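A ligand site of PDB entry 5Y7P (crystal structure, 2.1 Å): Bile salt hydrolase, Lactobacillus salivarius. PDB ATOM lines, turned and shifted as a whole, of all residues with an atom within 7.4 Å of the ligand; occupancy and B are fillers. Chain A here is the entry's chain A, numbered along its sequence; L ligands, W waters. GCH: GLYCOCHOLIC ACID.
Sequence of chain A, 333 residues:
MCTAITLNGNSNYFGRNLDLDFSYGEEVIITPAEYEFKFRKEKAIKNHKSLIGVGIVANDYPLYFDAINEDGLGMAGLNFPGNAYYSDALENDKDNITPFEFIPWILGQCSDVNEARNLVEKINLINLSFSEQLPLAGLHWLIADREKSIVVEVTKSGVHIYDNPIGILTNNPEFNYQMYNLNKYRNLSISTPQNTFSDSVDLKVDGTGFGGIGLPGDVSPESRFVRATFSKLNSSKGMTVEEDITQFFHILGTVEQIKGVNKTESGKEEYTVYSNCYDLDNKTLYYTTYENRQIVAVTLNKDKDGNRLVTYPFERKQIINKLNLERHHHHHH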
ATOM      1  N   PHE A  22      25.707   1.407 -13.587  1.00  0.00           N
ATOM      2  CA  PHE A  22      25.850   2.266 -12.405  1.00  0.00           C
ATOM      3  C   PHE A  22      25.352   1.511 -11.167  1.00  0.00           C
ATOM      4  O   PHE A  22      24.799   0.415 -11.282  1.00  0.00           O
ATOM      5  CB  PHE A  22      25.084   3.587 -12.581  1.00  0.00           C
ATOM      6  CG  PHE A  22      23.586   3.427 -12.669  1.00  0.00           C
ATOM      7  CD1 PHE A  22      22.974   3.119 -13.879  1.00  0.00           C
ATOM      8  CD2 PHE A  22      22.794   3.588 -11.539  1.00  0.00           C
ATOM      9  CE1 PHE A  22      21.590   2.966 -13.955  1.00  0.00           C
ATOM     10  CE2 PHE A  22      21.413   3.434 -11.605  1.00  0.00           C
ATOM     11  CZ  PHE A  22      20.813   3.133 -12.818  1.00  0.00           C
ATOM     12  N   SER A  23      25.550   2.102 -10.000  1.00  0.00           N
ATOM     13  CA  SER A  23      25.097   1.533  -8.729  1.00  0.00           C
ATOM     14  C   SER A  23      23.963   2.382  -8.148  1.00  0.00           C
ATOM     15  O   SER A  23      24.035   3.615  -8.153  1.00  0.00           O
ATOM     16  CB  SER A  23      26.255   1.454  -7.738  1.00  0.00           C
ATOM     17  OG  SER A  23      25.825   0.993  -6.464  1.00  0.00           O
ATOM     18  N   TYR A  24      22.928   1.717  -7.652  1.00  0.00           N
ATOM     19  CA  TYR A  24      21.823   2.380  -6.928  1.00  0.00           C
ATOM     20  C   TYR A  24      22.145   2.704  -5.463  1.00  0.00           C
ATOM     21  O   TYR A  24      21.326   3.311  -4.778  1.00  0.00           O
ATOM     22  CB  TYR A  24      20.552   1.513  -6.987  1.00  0.00           C
ATOM     23  CG  TYR A  24      19.735   1.665  -8.262  1.00  0.00           C
ATOM     24  CD1 TYR A  24      18.733   2.629  -8.352  1.00  0.00           C
ATOM     25  CD2 TYR A  24      19.963   0.840  -9.365  1.00  0.00           C
ATOM     26  CE1 TYR A  24      17.984   2.782  -9.509  1.00  0.00           C
ATOM     27  CE2 TYR A  24      19.211   0.983 -10.522  1.00  0.00           C
ATOM     28  CZ  TYR A  24      18.226   1.952 -10.595  1.00  0.00           C
ATOM     29  OH  TYR A  24      17.476   2.094 -11.743  1.00  0.00           O
ATOM     30  N   GLY A  25      23.329   2.312  -4.981  1.00  0.00           N
ATOM     31  CA  GLY A  25      23.626   2.372  -3.551  1.00  0.00           C
ATOM     32  C   GLY A  25      22.937   1.225  -2.854  1.00  0.00           C
ATOM     33  O   GLY A  25      22.182   1.416  -1.888  1.00  0.00           O
ATOM     34  N   GLU A  26      23.189   0.017  -3.361  1.00  0.00           N
ATOM     35  CA  GLU A  26      22.557  -1.221  -2.894  1.00  0.00           C
ATOM     36  C   GLU A  26      22.907  -1.502  -1.443  1.00  0.00           C
ATOM     37  O   GLU A  26      23.961  -1.090  -0.946  1.00  0.00           O
ATOM     38  CB  GLU A  26      22.993  -2.433  -3.731  1.00  0.00           C
ATOM     39  CG  GLU A  26      22.605  -2.423  -5.215  1.00  0.00           C
ATOM     40  CD  GLU A  26      23.480  -1.532  -6.086  1.00  0.00           C
ATOM     41  OE1 GLU A  26      24.671  -1.340  -5.779  1.00  0.00           O
ATOM     42  OE2 GLU A  26      22.962  -1.010  -7.099  1.00  0.00           O
ATOM     43  N   GLU A  27      22.018  -2.222  -0.762  1.00  0.00           N
ATOM     44  CA  GLU A  27      22.221  -2.583   0.640  1.00  0.00           C
ATOM     45  C   GLU A  27      21.481  -3.862   1.007  1.00  0.00           C
ATOM     46  O   GLU A  27      20.532  -4.254   0.328  1.00  0.00           O
ATOM     47  CB  GLU A  27      21.757  -1.436   1.562  1.00  0.00           C
ATOM     48  CG  GLU A  27      20.249  -1.226   1.611  1.00  0.00           C
ATOM     49  CD  GLU A  27      19.870   0.146   2.144  1.00  0.00           C
ATOM     50  OE1 GLU A  27      20.525   0.628   3.097  1.00  0.00           O
ATOM     51  OE2 GLU A  27      18.912   0.750   1.619  1.00  0.00           O
ATOM     52  N   ILE A  29      18.811  -5.583   3.064  1.00  0.00           N
ATOM     53  CA  ILE A  29      17.564  -5.169   3.713  1.00  0.00           C
ATOM     54  C   ILE A  29      16.917  -6.402   4.350  1.00  0.00           C
ATOM     55  O   ILE A  29      16.623  -7.381   3.666  1.00  0.00           O
ATOM     56  CB  ILE A  29      16.555  -4.529   2.717  1.00  0.00           C
ATOM     57  CG1 ILE A  29      17.198  -3.368   1.961  1.00  0.00           C
ATOM     58  CG2 ILE A  29      15.315  -4.034   3.453  1.00  0.00           C
ATOM     59  CD1 ILE A  29      16.471  -2.993   0.680  1.00  0.00           C
ATOM     60  N   GLY A  55      18.803  -4.736  -2.101  1.00  0.00           N
ATOM     61  CA  GLY A  55      18.034  -3.730  -2.811  1.00  0.00           C
ATOM     62  C   GLY A  55      18.300  -2.325  -2.293  1.00  0.00           C
ATOM     63  O   GLY A  55      19.372  -2.055  -1.771  1.00  0.00           O
ATOM     64  N   ILE A  56      17.314  -1.449  -2.457  1.00  0.00           N
ATOM     65  CA  ILE A  56      17.334  -0.105  -1.867  1.00  0.00           C
ATOM     66  C   ILE A  56      16.019   0.152  -1.139  1.00  0.00           C
ATOM     67  O   ILE A  56      14.978  -0.420  -1.497  1.00  0.00           O
ATOM     68  CB  ILE A  56      17.597   0.993  -2.931  1.00  0.00           C
ATOM     69  CG1 ILE A  56      16.511   1.008  -4.019  1.00  0.00           C
ATOM     70  CG2 ILE A  56      18.970   0.792  -3.555  1.00  0.00           C
ATOM     71  CD1 ILE A  56      16.598   2.192  -4.955  1.00  0.00           C
ATOM     72  N   VAL A  57      16.066   0.987  -0.109  1.00  0.00           N
ATOM     73  CA  VAL A  57      14.868   1.459   0.572  1.00  0.00           C
ATOM     74  C   VAL A  57      14.488   2.828  -0.006  1.00  0.00           C
ATOM     75  O   VAL A  57      15.342   3.717  -0.092  1.00  0.00           O
ATOM     76  CB  VAL A  57      15.079   1.566   2.103  1.00  0.00           C
ATOM     77  CG1 VAL A  57      13.775   1.965   2.797  1.00  0.00           C
ATOM     78  CG2 VAL A  57      15.583   0.253   2.673  1.00  0.00           C
ATOM     79  N   ALA A  58      13.233   2.980  -0.404  1.00  0.00           N
ATOM     80  CA  ALA A  58      12.695   4.262  -0.873  1.00  0.00           C
ATOM     81  C   ALA A  58      11.318   4.485  -0.246  1.00  0.00           C
ATOM     82  O   ALA A  58      10.488   3.588  -0.250  1.00  0.00           O
ATOM     83  CB  ALA A  58      12.591   4.279  -2.392  1.00  0.00           C
ATOM     84  N   ASN A  59      11.099   5.682   0.313  1.00  0.00           N
ATOM     85  CA  ASN A  59       9.884   6.024   1.072  1.00  0.00           C
ATOM     86  C   ASN A  59       9.528   4.954   2.122  1.00  0.00           C
ATOM     87  O   ASN A  59       8.361   4.558   2.259  1.00  0.00           O
ATOM     88  CB  ASN A  59       8.711   6.275   0.110  1.00  0.00           C
ATOM     89  CG  ASN A  59       7.560   7.035   0.760  1.00  0.00           C
ATOM     90  OD1 ASN A  59       7.748   7.817   1.696  1.00  0.00           O
ATOM     91  ND2 ASN A  59       6.348   6.829   0.250  1.00  0.00           N
ATOM     92  N   ASP A  60      10.548   4.477   2.838  1.00  0.00           N
ATOM     93  CA  ASP A  60      10.417   3.411   3.837  1.00  0.00           C
ATOM     94  C   ASP A  60       9.875   2.080   3.264  1.00  0.00           C
ATOM     95  O   ASP A  60       9.303   1.274   4.008  1.00  0.00           O
ATOM     96  CB  ASP A  60       9.535   3.903   5.017  1.00  0.00           C
ATOM     97  CG  ASP A  60       9.659   3.042   6.265  1.00  0.00           C
ATOM     98  OD1 ASP A  60      10.789   2.699   6.661  1.00  0.00           O
ATOM     99  OD2 ASP A  60       8.616   2.714   6.863  1.00  0.00           O
ATOM    100  N   LEU A  63      12.678  -2.050  -1.714  1.00  0.00           N
ATOM    101  CA  LEU A  63      12.664  -2.364  -3.137  1.00  0.00           C
ATOM    102  C   LEU A  63      13.715  -3.428  -3.442  1.00  0.00           C
ATOM    103  O   LEU A  63      14.846  -3.104  -3.814  1.00  0.00           O
ATOM    104  CB  LEU A  63      12.912  -1.103  -3.976  1.00  0.00           C
ATOM    105  CG  LEU A  63      11.800  -0.053  -3.977  1.00  0.00           C
ATOM    106  CD1 LEU A  63      12.275   1.254  -4.572  1.00  0.00           C
ATOM    107  CD2 LEU A  63      10.577  -0.560  -4.727  1.00  0.00           C
ATOM    108  N   PHE A 130       6.697   2.892  -9.183  1.00  0.00           N
ATOM    109  CA  PHE A 130       6.905   3.209  -7.770  1.00  0.00           C
ATOM    110  C   PHE A 130       6.822   4.719  -7.555  1.00  0.00           C
ATOM    111  O   PHE A 130       6.121   5.176  -6.645  1.00  0.00           O
ATOM    112  CB  PHE A 130       8.265   2.680  -7.285  1.00  0.00           C
ATOM    113  CG  PHE A 130       8.544   2.996  -5.850  1.00  0.00           C
ATOM    114  CD1 PHE A 130       7.984   2.218  -4.837  1.00  0.00           C
ATOM    115  CD2 PHE A 130       9.338   4.082  -5.499  1.00  0.00           C
ATOM    116  CE1 PHE A 130       8.238   2.510  -3.500  1.00  0.00           C
ATOM    117  CE2 PHE A 130       9.582   4.387  -4.170  1.00  0.00           C
ATOM    118  CZ  PHE A 130       9.035   3.595  -3.172  1.00  0.00           C
ATOM    119  N   SER A 131       7.549   5.468  -8.377  1.00  0.00           N
ATOM    120  CA  SER A 131       7.572   6.924  -8.298  1.00  0.00           C
ATOM    121  C   SER A 131       8.122   7.516  -9.594  1.00  0.00           C
ATOM    122  O   SER A 131       8.509   6.779 -10.504  1.00  0.00           O
ATOM    123  CB  SER A 131       8.428   7.377  -7.111  1.00  0.00           C
ATOM    124  OG  SER A 131       9.786   7.025  -7.297  1.00  0.00           O
ATOM    125  N   GLN A 133      10.902   9.313  -9.731  1.00  0.00           N
ATOM    126  CA  GLN A 133      12.346   9.060  -9.652  1.00  0.00           C
ATOM    127  C   GLN A 133      12.736   7.634 -10.058  1.00  0.00           C
ATOM    128  O   GLN A 133      13.794   7.435 -10.649  1.00  0.00           O
ATOM    129  CB  GLN A 133      12.840   9.342  -8.226  1.00  0.00           C
ATOM    130  CG  GLN A 133      14.350   9.185  -7.990  1.00  0.00           C
ATOM    131  CD  GLN A 133      15.197  10.284  -8.619  1.00  0.00           C
ATOM    132  OE1 GLN A 133      14.679  11.204  -9.268  1.00  0.00           O
ATOM    133  NE2 GLN A 133      16.508  10.198  -8.428  1.00  0.00           N
ATOM    134  N   LEU A 134      11.886   6.660  -9.719  1.00  0.00           N
ATOM    135  CA  LEU A 134      12.182   5.241  -9.933  1.00  0.00           C
ATOM    136  C   LEU A 134      11.106   4.595 -10.816  1.00  0.00           C
ATOM    137  O   LEU A 134      10.209   3.908 -10.307  1.00  0.00           O
ATOM    138  CB  LEU A 134      12.288   4.533  -8.574  1.00  0.00           C
ATOM    139  CG  LEU A 134      13.362   5.075  -7.625  1.00  0.00           C
ATOM    140  CD1 LEU A 134      13.140   4.582  -6.203  1.00  0.00           C
ATOM    141  CD2 LEU A 134      14.758   4.711  -8.113  1.00  0.00           C
ATOM    142  N   PRO A 135      11.182   4.809 -12.149  1.00  0.00           N
ATOM    143  CA  PRO A 135      10.169   4.248 -13.053  1.00  0.00           C
ATOM    144  C   PRO A 135      10.340   2.752 -13.280  1.00  0.00           C
ATOM    145  O   PRO A 135      11.391   2.192 -12.964  1.00  0.00           O
ATOM    146  CB  PRO A 135      10.383   5.026 -14.357  1.00  0.00           C
ATOM    147  CG  PRO A 135      11.747   5.614 -14.283  1.00  0.00           C
ATOM    148  CD  PRO A 135      12.293   5.430 -12.897  1.00  0.00           C
ATOM    149  N   THR A 311      18.743  -2.423   7.904  1.00  0.00           N
ATOM    150  CA  THR A 311      19.571  -2.261   6.707  1.00  0.00           C
ATOM    151  C   THR A 311      21.069  -2.215   7.024  1.00  0.00           C
ATOM    152  O   THR A 311      21.481  -1.680   8.057  1.00  0.00           O
ATOM    153  CB  THR A 311      19.191  -0.986   5.934  1.00  0.00           C
ATOM    154  OG1 THR A 311      19.294   0.156   6.797  1.00  0.00           O
ATOM    155  CG2 THR A 311      17.765  -1.096   5.406  1.00  0.00           C
ATOM    156  N   TYR A 312      21.864  -2.805   6.130  1.00  0.00           N
ATOM    157  CA  TYR A 312      23.331  -2.751   6.186  1.00  0.00           C
ATOM    158  C   TYR A 312      23.850  -2.327   4.813  1.00  0.00           C
ATOM    159  O   TYR A 312      23.807  -3.122   3.868  1.00  0.00           O
ATOM    160  CB  TYR A 312      23.913  -4.119   6.564  1.00  0.00           C
ATOM    161  CG  TYR A 312      23.401  -4.671   7.873  1.00  0.00           C
ATOM    162  CD1 TYR A 312      24.032  -4.369   9.078  1.00  0.00           C
ATOM    163  CD2 TYR A 312      22.286  -5.512   7.909  1.00  0.00           C
ATOM    164  CE1 TYR A 312      23.566  -4.882  10.284  1.00  0.00           C
ATOM    165  CE2 TYR A 312      21.815  -6.034   9.106  1.00  0.00           C
ATOM    166  CZ  TYR A 312      22.455  -5.714  10.289  1.00  0.00           C
ATOM    167  OH  TYR A 312      21.987  -6.227  11.485  1.00  0.00           O
ATOM    168  N   PRO A 313      24.314  -1.068   4.674  1.00  0.00           N
ATOM    169  CA  PRO A 313      24.844  -0.617   3.383  1.00  0.00           C
ATOM    170  C   PRO A 313      26.116  -1.351   2.930  1.00  0.00           C
ATOM    171  O   PRO A 313      26.931  -1.754   3.759  1.00  0.00           O
ATOM    172  CB  PRO A 313      25.141   0.872   3.619  1.00  0.00           C
ATOM    173  CG  PRO A 313      24.241   1.265   4.733  1.00  0.00           C
ATOM    174  CD  PRO A 313      24.196   0.058   5.615  1.00  0.00           C
HETATM  175  C   GCH L   1      19.569   9.142 -11.330  1.00  0.00           C
HETATM  176  O   GCH L   1      18.854  10.268 -11.796  1.00  0.00           O
HETATM  177  C1  GCH L   1      20.533   9.592 -10.256  1.00  0.00           C
HETATM  178  C2  GCH L   1      21.300   8.398  -9.653  1.00  0.00           C
HETATM  179  C3  GCH L   1      20.381   7.247  -9.217  1.00  0.00           C
HETATM  180  C4  GCH L   1      19.395   6.897 -10.361  1.00  0.00           C
HETATM  181  C5  GCH L   1      18.567   8.068 -10.886  1.00  0.00           C
HETATM  182  C6  GCH L   1      21.240   5.992  -8.977  1.00  0.00           C
HETATM  183  C7  GCH L   1      22.225   8.924  -8.531  1.00  0.00           C
HETATM  184  C8  GCH L   1      21.501   9.200  -7.213  1.00  0.00           C
HETATM  185  O1  GCH L   1      20.750  10.433  -7.318  1.00  0.00           O
HETATM  186  C9  GCH L   1      20.553   8.038  -6.791  1.00  0.00           C
HETATM  187  C10 GCH L   1      19.609   7.685  -7.936  1.00  0.00           C
HETATM  188  C11 GCH L   1      18.502   6.686  -7.520  1.00  0.00           C
HETATM  189  C12 GCH L   1      17.807   6.943  -6.160  1.00  0.00           C
HETATM  190  C13 GCH L   1      18.813   7.214  -5.048  1.00  0.00           C
HETATM  191  C14 GCH L   1      19.714   8.370  -5.552  1.00  0.00           C
HETATM  192  C15 GCH L   1      20.465   8.803  -4.297  1.00  0.00           C
HETATM  193  C16 GCH L   1      19.422   8.601  -3.201  1.00  0.00           C
HETATM  194  C17 GCH L   1      18.265   7.792  -3.744  1.00  0.00           C
HETATM  195  C18 GCH L   1      17.621   6.873  -2.688  1.00  0.00           C
HETATM  196  C19 GCH L   1      16.429   6.075  -3.251  1.00  0.00           C
HETATM  197  C20 GCH L   1      17.071   7.755  -1.556  1.00  0.00           C
HETATM  198  C21 GCH L   1      16.582   7.102  -0.250  1.00  0.00           C
HETATM  199  C22 GCH L   1      17.727   6.284   0.249  1.00  0.00           C
HETATM  200  N   GCH L   1      17.585   4.968   0.214  1.00  0.00           N
HETATM  201  CA  GCH L   1      18.663   4.022   0.430  1.00  0.00           C
HETATM  202  O2  GCH L   1      18.766   6.846   0.502  1.00  0.00           O
HETATM  203  C23 GCH L   1      19.669   5.981  -4.733  1.00  0.00           C
HETATM  204  O3  GCH L   1      16.906   8.054  -6.390  1.00  0.00           O
HETATM  205  C24 GCH L   1      19.131   4.051   1.885  1.00  0.00           C
HETATM  206  O4  GCH L   1      18.454   4.605   2.776  1.00  0.00           O
HETATM  207  O5  GCH L   1      20.208   3.514   2.155  1.00  0.00           O
HETATM  208  O   HOH W   1      19.241   8.786   2.170  1.00  0.00           O
HETATM  209  O   HOH W   2      16.073   4.904   3.493  1.00  0.00           O
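Phe 22 touches the ligand. Ser 23 touches the ligand (O to C6, 3.8 Å). Tyr 24 touches the ligand (O to C23, 3.1 Å). The nearest printed residue that does not touch the ligand is Ile 56 (4.2 Å).
The backbone NH (N) of Val 57 sits at hydrogen-bond distance from the side-chain carboxylate (OE2) of Glu 27. The side-chain hydroxyl (OG) of Ser 23 is in hydrogen-bond range of the side-chain carboxylate (OE1) of Glu 26, at 2.7 Å. The backbone NH of Glu 27 lies within hydrogen-bond range of the backbone carbonyl oxygen of Gly 55. The backbone NH (N) of Gly 25 is in hydrogen-bond range of the side-chain hydroxyl (OG) of Ser 23 (3.2 Å). The backbone NH (N) of Tyr 24 sits at hydrogen-bond distance from the side-chain carboxylate (OE2) of Glu 26, 2.8 Å away.
The side-chain amide nitrogen of Gln 133 lies within hydrogen-bond range of an oxygen (O3) of the ligand, at 3.0 Å. OE1 of Glu 27 lies close to O5 of the ligand, 3.1 Å away. O of Val 57 is in hydrogen-bond range of N of the ligand (2.6 Å).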
